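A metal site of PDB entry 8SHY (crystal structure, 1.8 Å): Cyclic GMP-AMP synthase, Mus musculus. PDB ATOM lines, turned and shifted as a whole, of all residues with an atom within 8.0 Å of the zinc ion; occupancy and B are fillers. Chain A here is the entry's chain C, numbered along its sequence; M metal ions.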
ATOM      1  N   LEU A 232     -21.542  28.927   1.926  1.00  0.00           N
ATOM      2  CA  LEU A 232     -21.732  29.566   3.245  1.00  0.00           C
ATOM      3  C   LEU A 232     -22.577  28.709   4.169  1.00  0.00           C
ATOM      4  O   LEU A 232     -22.331  28.682   5.391  1.00  0.00           O
ATOM      5  CB  LEU A 232     -22.377  30.945   3.107  1.00  0.00           C
ATOM      6  CG  LEU A 232     -21.462  32.173   3.089  1.00  0.00           C
ATOM      7  CD1 LEU A 232     -20.876  32.384   4.453  1.00  0.00           C
ATOM      8  CD2 LEU A 232     -20.363  32.014   2.092  1.00  0.00           C
ATOM      9  N   ASN A 233     -23.565  28.016   3.638  1.00  0.00           N
ATOM     10  CA  ASN A 233     -24.448  27.238   4.487  1.00  0.00           C
ATOM     11  C   ASN A 233     -24.015  25.780   4.639  1.00  0.00           C
ATOM     12  O   ASN A 233     -24.610  25.052   5.428  1.00  0.00           O
ATOM     13  CB  ASN A 233     -25.886  27.325   3.950  1.00  0.00           C
ATOM     14  CG  ASN A 233     -26.483  28.731   4.125  1.00  0.00           C
ATOM     15  OD1 ASN A 233     -25.976  29.540   4.930  1.00  0.00           O
ATOM     16  ND2 ASN A 233     -27.516  29.045   3.344  1.00  0.00           N
ATOM     17  N   ASN A 234     -22.962  25.361   3.923  1.00  0.00           N
ATOM     18  CA  ASN A 234     -22.437  24.005   3.970  1.00  0.00           C
ATOM     19  C   ASN A 234     -20.915  24.105   4.017  1.00  0.00           C
ATOM     20  O   ASN A 234     -20.205  23.632   3.140  1.00  0.00           O
ATOM     21  CB  ASN A 234     -22.874  23.193   2.751  1.00  0.00           C
ATOM     22  CG  ASN A 234     -24.378  23.037   2.664  1.00  0.00           C
ATOM     23  OD1 ASN A 234     -24.940  22.051   3.150  1.00  0.00           O
ATOM     24  ND2 ASN A 234     -25.053  24.025   2.055  1.00  0.00           N
ATOM     25  N   HIS A 235     -20.399  24.764   5.046  1.00  0.00           N
ATOM     26  CA  HIS A 235     -19.042  25.296   5.003  1.00  0.00           C
ATOM     27  C   HIS A 235     -18.016  24.420   5.722  1.00  0.00           C
ATOM     28  O   HIS A 235     -16.853  24.811   5.788  1.00  0.00           O
ATOM     29  CB  HIS A 235     -19.019  26.663   5.644  1.00  0.00           C
ATOM     30  CG  HIS A 235     -19.574  26.643   7.030  1.00  0.00           C
ATOM     31  ND1 HIS A 235     -20.743  27.284   7.373  1.00  0.00           N
ATOM     32  CD2 HIS A 235     -19.155  25.995   8.143  1.00  0.00           C
ATOM     33  CE1 HIS A 235     -21.013  27.050   8.658  1.00  0.00           C
ATOM     34  NE2 HIS A 235     -20.064  26.267   9.138  1.00  0.00           N
ATOM     35  N   GLY A 236     -18.432  23.293   6.311  1.00  0.00           N
ATOM     36  CA  GLY A 236     -17.525  22.485   7.108  1.00  0.00           C
ATOM     37  C   GLY A 236     -16.924  21.311   6.346  1.00  0.00           C
ATOM     38  O   GLY A 236     -17.449  20.849   5.332  1.00  0.00           O
ATOM     39  N   ILE A 237     -15.793  20.818   6.847  1.00  0.00           N
ATOM     40  CA  ILE A 237     -15.332  19.545   6.315  1.00  0.00           C
ATOM     41  C   ILE A 237     -16.233  18.426   6.812  1.00  0.00           C
ATOM     42  O   ILE A 237     -16.502  17.456   6.093  1.00  0.00           O
ATOM     43  CB  ILE A 237     -13.839  19.331   6.674  1.00  0.00           C
ATOM     44  CG1 ILE A 237     -13.184  18.306   5.754  1.00  0.00           C
ATOM     45  CG2 ILE A 237     -13.682  19.001   8.155  1.00  0.00           C
ATOM     46  CD1 ILE A 237     -11.666  18.266   5.889  1.00  0.00           C
ATOM     47  N   GLU A 238     -16.775  18.564   8.025  1.00  0.00           N
ATOM     48  CA  GLU A 238     -17.774  17.639   8.519  1.00  0.00           C
ATOM     49  C   GLU A 238     -19.153  18.104   8.087  1.00  0.00           C
ATOM     50  O   GLU A 238     -19.467  19.305   8.110  1.00  0.00           O
ATOM     51  CB  GLU A 238     -17.700  17.511  10.041  1.00  0.00           C
ATOM     52  CG  GLU A 238     -16.464  16.750  10.511  1.00  0.00           C
ATOM     53  CD  GLU A 238     -16.556  16.369  11.977  1.00  0.00           C
ATOM     54  OE1 GLU A 238     -17.684  16.279  12.499  1.00  0.00           O
ATOM     55  OE2 GLU A 238     -15.512  16.070  12.589  1.00  0.00           O
ATOM     56  N   THR A 240     -21.910  17.761   9.497  1.00  0.00           N
ATOM     57  CA  THR A 240     -22.712  18.197  10.626  1.00  0.00           C
ATOM     58  C   THR A 240     -22.250  19.532  11.194  1.00  0.00           C
ATOM     59  O   THR A 240     -22.821  19.968  12.199  1.00  0.00           O
ATOM     60  CB  THR A 240     -22.688  17.141  11.727  1.00  0.00           C
ATOM     61  OG1 THR A 240     -21.345  16.835  12.082  1.00  0.00           O
ATOM     62  CG2 THR A 240     -23.391  15.859  11.288  1.00  0.00           C
ATOM     63  N   CYS A 241     -21.249  20.168  10.595  1.00  0.00           N
ATOM     64  CA  CYS A 241     -20.726  21.438  11.097  1.00  0.00           C
ATOM     65  C   CYS A 241     -21.843  22.463  11.254  1.00  0.00           C
ATOM     66  O   CYS A 241     -22.582  22.752  10.288  1.00  0.00           O
ATOM     67  CB  CYS A 241     -19.638  21.968  10.171  1.00  0.00           C
ATOM     68  SG  CYS A 241     -18.665  23.392  10.879  1.00  0.00           S
ATOM     69  N   CYS A 242     -21.973  22.984  12.473  1.00  0.00           N
ATOM     70  CA  CYS A 242     -22.997  23.953  12.862  1.00  0.00           C
ATOM     71  C   CYS A 242     -24.423  23.403  12.762  1.00  0.00           C
ATOM     72  O   CYS A 242     -25.380  24.186  12.749  1.00  0.00           O
ATOM     73  CB  CYS A 242     -22.875  25.250  12.051  1.00  0.00           C
ATOM     74  SG  CYS A 242     -21.383  26.201  12.391  1.00  0.00           S
ATOM     75  N   GLU A 243     -24.608  22.091  12.707  1.00  0.00           N
ATOM     76  CA  GLU A 243     -25.961  21.549  12.772  1.00  0.00           C
ATOM     77  C   GLU A 243     -26.323  21.184  14.212  1.00  0.00           C
ATOM     78  O   GLU A 243     -25.482  21.158  15.105  1.00  0.00           O
ATOM     79  CB  GLU A 243     -26.125  20.319  11.888  1.00  0.00           C
ATOM     80  CG  GLU A 243     -26.071  20.584  10.395  1.00  0.00           C
ATOM     81  CD  GLU A 243     -26.313  19.311   9.601  1.00  0.00           C
ATOM     82  OE1 GLU A 243     -26.344  18.236  10.232  1.00  0.00           O
ATOM     83  OE2 GLU A 243     -26.476  19.392   8.367  1.00  0.00           O
ATOM     84  N   ALA A 247     -21.032  20.103  15.732  1.00  0.00           N
ATOM     85  CA  ALA A 247     -20.277  21.084  16.493  1.00  0.00           C
ATOM     86  C   ALA A 247     -20.299  22.444  15.794  1.00  0.00           C
ATOM     87  O   ALA A 247     -20.123  22.526  14.581  1.00  0.00           O
ATOM     88  CB  ALA A 247     -18.830  20.641  16.665  1.00  0.00           C
ATOM     89  N   LYS A 248     -20.506  23.505  16.576  1.00  0.00           N
ATOM     90  CA  LYS A 248     -20.356  24.863  16.062  1.00  0.00           C
ATOM     91  C   LYS A 248     -18.905  25.143  15.676  1.00  0.00           C
ATOM     92  O   LYS A 248     -17.976  24.644  16.302  1.00  0.00           O
ATOM     93  CB  LYS A 248     -20.800  25.887  17.104  1.00  0.00           C
ATOM     94  CG  LYS A 248     -22.276  26.197  17.126  1.00  0.00           C
ATOM     95  CD  LYS A 248     -22.663  26.886  15.829  1.00  0.00           C
ATOM     96  CE  LYS A 248     -22.290  28.372  15.880  1.00  0.00           C
ATOM     97  NZ  LYS A 248     -22.030  28.955  14.514  1.00  0.00           N
ATOM     98  N   CYS A 249     -18.719  25.973  14.647  1.00  0.00           N
ATOM     99  CA  CYS A 249     -17.431  26.584  14.287  1.00  0.00           C
ATOM    100  C   CYS A 249     -17.611  28.104  14.257  1.00  0.00           C
ATOM    101  O   CYS A 249     -18.724  28.626  14.407  1.00  0.00           O
ATOM    102  CB  CYS A 249     -16.930  26.074  12.928  1.00  0.00           C
ATOM    103  SG  CYS A 249     -17.782  26.827  11.490  1.00  0.00           S
ATOM    104  N   CYS A 250     -16.499  28.848  14.076  1.00  0.00           N
ATOM    105  CA  CYS A 250     -16.569  30.302  14.031  1.00  0.00           C
ATOM    106  C   CYS A 250     -16.359  30.884  12.629  1.00  0.00           C
ATOM    107  O   CYS A 250     -16.046  32.073  12.494  1.00  0.00           O
ATOM    108  CB  CYS A 250     -15.578  30.942  15.010  1.00  0.00           C
ATOM    109  SG  CYS A 250     -13.830  30.669  14.603  1.00  0.00           S
ATOM    110  N   ARG A 251     -16.557  30.077  11.589  1.00  0.00           N
ATOM    111  CA  ARG A 251     -16.313  30.550  10.219  1.00  0.00           C
ATOM    112  C   ARG A 251     -17.188  31.749   9.864  1.00  0.00           C
ATOM    113  O   ARG A 251     -16.683  32.778   9.396  1.00  0.00           O
ATOM    114  CB  ARG A 251     -16.542  29.403   9.230  1.00  0.00           C
ATOM    115  CG  ARG A 251     -15.398  28.365   9.208  1.00  0.00           C
ATOM    116  CD  ARG A 251     -15.591  27.411   8.017  1.00  0.00           C
ATOM    117  NE  ARG A 251     -14.577  26.358   7.920  1.00  0.00           N
ATOM    118  CZ  ARG A 251     -14.731  25.154   8.437  1.00  0.00           C
ATOM    119  NH1 ARG A 251     -15.742  24.862   9.253  1.00  0.00           N
ATOM    120  NH2 ARG A 251     -13.862  24.188   8.119  1.00  0.00           N
ATOM    121  N   LYS A 252     -18.508  31.631  10.025  1.00  0.00           N
ATOM    122  CA  LYS A 252     -19.396  32.729   9.652  1.00  0.00           C
ATOM    123  C   LYS A 252     -19.238  33.911  10.601  1.00  0.00           C
ATOM    124  O   LYS A 252     -19.388  35.068  10.172  1.00  0.00           O
ATOM    125  CB  LYS A 252     -20.838  32.224   9.613  1.00  0.00           C
ATOM    126  CG  LYS A 252     -21.071  31.138   8.544  1.00  0.00           C
ATOM    127  CD  LYS A 252     -22.525  30.634   8.463  1.00  0.00           C
ATOM    128  CE  LYS A 252     -23.373  31.406   7.484  1.00  0.00           C
ATOM    129  NZ  LYS A 252     -24.705  30.701   7.315  1.00  0.00           N
ATOM    130  N   GLU A 253     -18.927  33.647  11.875  1.00  0.00           N
ATOM    131  CA  GLU A 253     -18.645  34.730  12.819  1.00  0.00           C
ATOM    132  C   GLU A 253     -17.460  35.587  12.362  1.00  0.00           C
ATOM    133  O   GLU A 253     -17.518  36.816  12.444  1.00  0.00           O
ATOM    134  CB  GLU A 253     -18.435  34.152  14.225  1.00  0.00           C
ATOM    135  CG  GLU A 253     -19.682  33.517  14.828  1.00  0.00           C
ATOM    136  CD  GLU A 253     -20.170  32.217  14.208  1.00  0.00           C
ATOM    137  OE1 GLU A 253     -19.467  31.582  13.378  1.00  0.00           O
ATOM    138  OE2 GLU A 253     -21.312  31.820  14.582  1.00  0.00           O
ATOM    139  N   ASP A 294     -12.344  21.758  10.369  1.00  0.00           N
ATOM    140  CA  ASP A 294     -13.285  22.384  11.303  1.00  0.00           C
ATOM    141  C   ASP A 294     -12.613  22.719  12.624  1.00  0.00           C
ATOM    142  O   ASP A 294     -12.947  23.721  13.254  1.00  0.00           O
ATOM    143  CB  ASP A 294     -14.478  21.474  11.556  1.00  0.00           C
ATOM    144  CG  ASP A 294     -15.298  21.243  10.303  1.00  0.00           C
ATOM    145  OD1 ASP A 294     -15.087  21.986   9.306  1.00  0.00           O
ATOM    146  OD2 ASP A 294     -16.147  20.339  10.343  1.00  0.00           O
ATOM    147  N   TRP A 297     -11.284  26.108  13.113  1.00  0.00           N
ATOM    148  CA  TRP A 297     -12.299  27.143  13.317  1.00  0.00           C
ATOM    149  C   TRP A 297     -13.158  26.847  14.550  1.00  0.00           C
ATOM    150  O   TRP A 297     -14.358  27.131  14.576  1.00  0.00           O
ATOM    151  CB  TRP A 297     -13.146  27.265  12.039  1.00  0.00           C
ATOM    152  CG  TRP A 297     -12.268  27.640  10.897  1.00  0.00           C
ATOM    153  CD1 TRP A 297     -11.568  26.792  10.087  1.00  0.00           C
ATOM    154  CD2 TRP A 297     -11.961  28.966  10.425  1.00  0.00           C
ATOM    155  NE1 TRP A 297     -10.847  27.501   9.155  1.00  0.00           N
ATOM    156  CE2 TRP A 297     -11.075  28.840   9.340  1.00  0.00           C
ATOM    157  CE3 TRP A 297     -12.355  30.253  10.832  1.00  0.00           C
ATOM    158  CZ2 TRP A 297     -10.558  29.944   8.643  1.00  0.00           C
ATOM    159  CZ3 TRP A 297     -11.854  31.350  10.134  1.00  0.00           C
ATOM    160  CH2 TRP A 297     -10.975  31.184   9.036  1.00  0.00           C
HETATM  161 ZN    ZN M   1     -19.662  25.505  11.017  1.00  0.00          ZN
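Within 4 Å of the zinc ion: His 235, Cys 241, Cys 242 and Cys 249.
O of His 235 sits close to NE of Arg 251, 3.5 Å away. The backbone carbonyl oxygen (O) of Leu 232 sits at hydrogen-bond distance from a ring nitrogen (ND1) of His 235, 2.9 Å away. The backbone NH (N) of Cys 242 lies within hydrogen-bond range of the backbone carbonyl oxygen (O) of Ala 247 (2.8 Å). The side-chain amino group of Lys 248 lies close to the side-chain sulfur of Cys 242. The side-chain sulfur (SG) of Cys 241 lies close to the guanidinium group (NH1) of Arg 251, at 3.7 Å. The side-chain sulfur of Cys 249 lies close to the backbone NH of Arg 251 (3.5 Å).
The zinc ion is bound by a ring nitrogen (NE2) of His 235 (2.1 Å), the side-chain sulfur of Cys 242 (2.3 Å), the side-chain sulfur of Cys 241 (2.3 Å) and the side-chain sulfur of Cys 249 (2.3 Å). The zinc ion has four donor atoms within binding distance.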
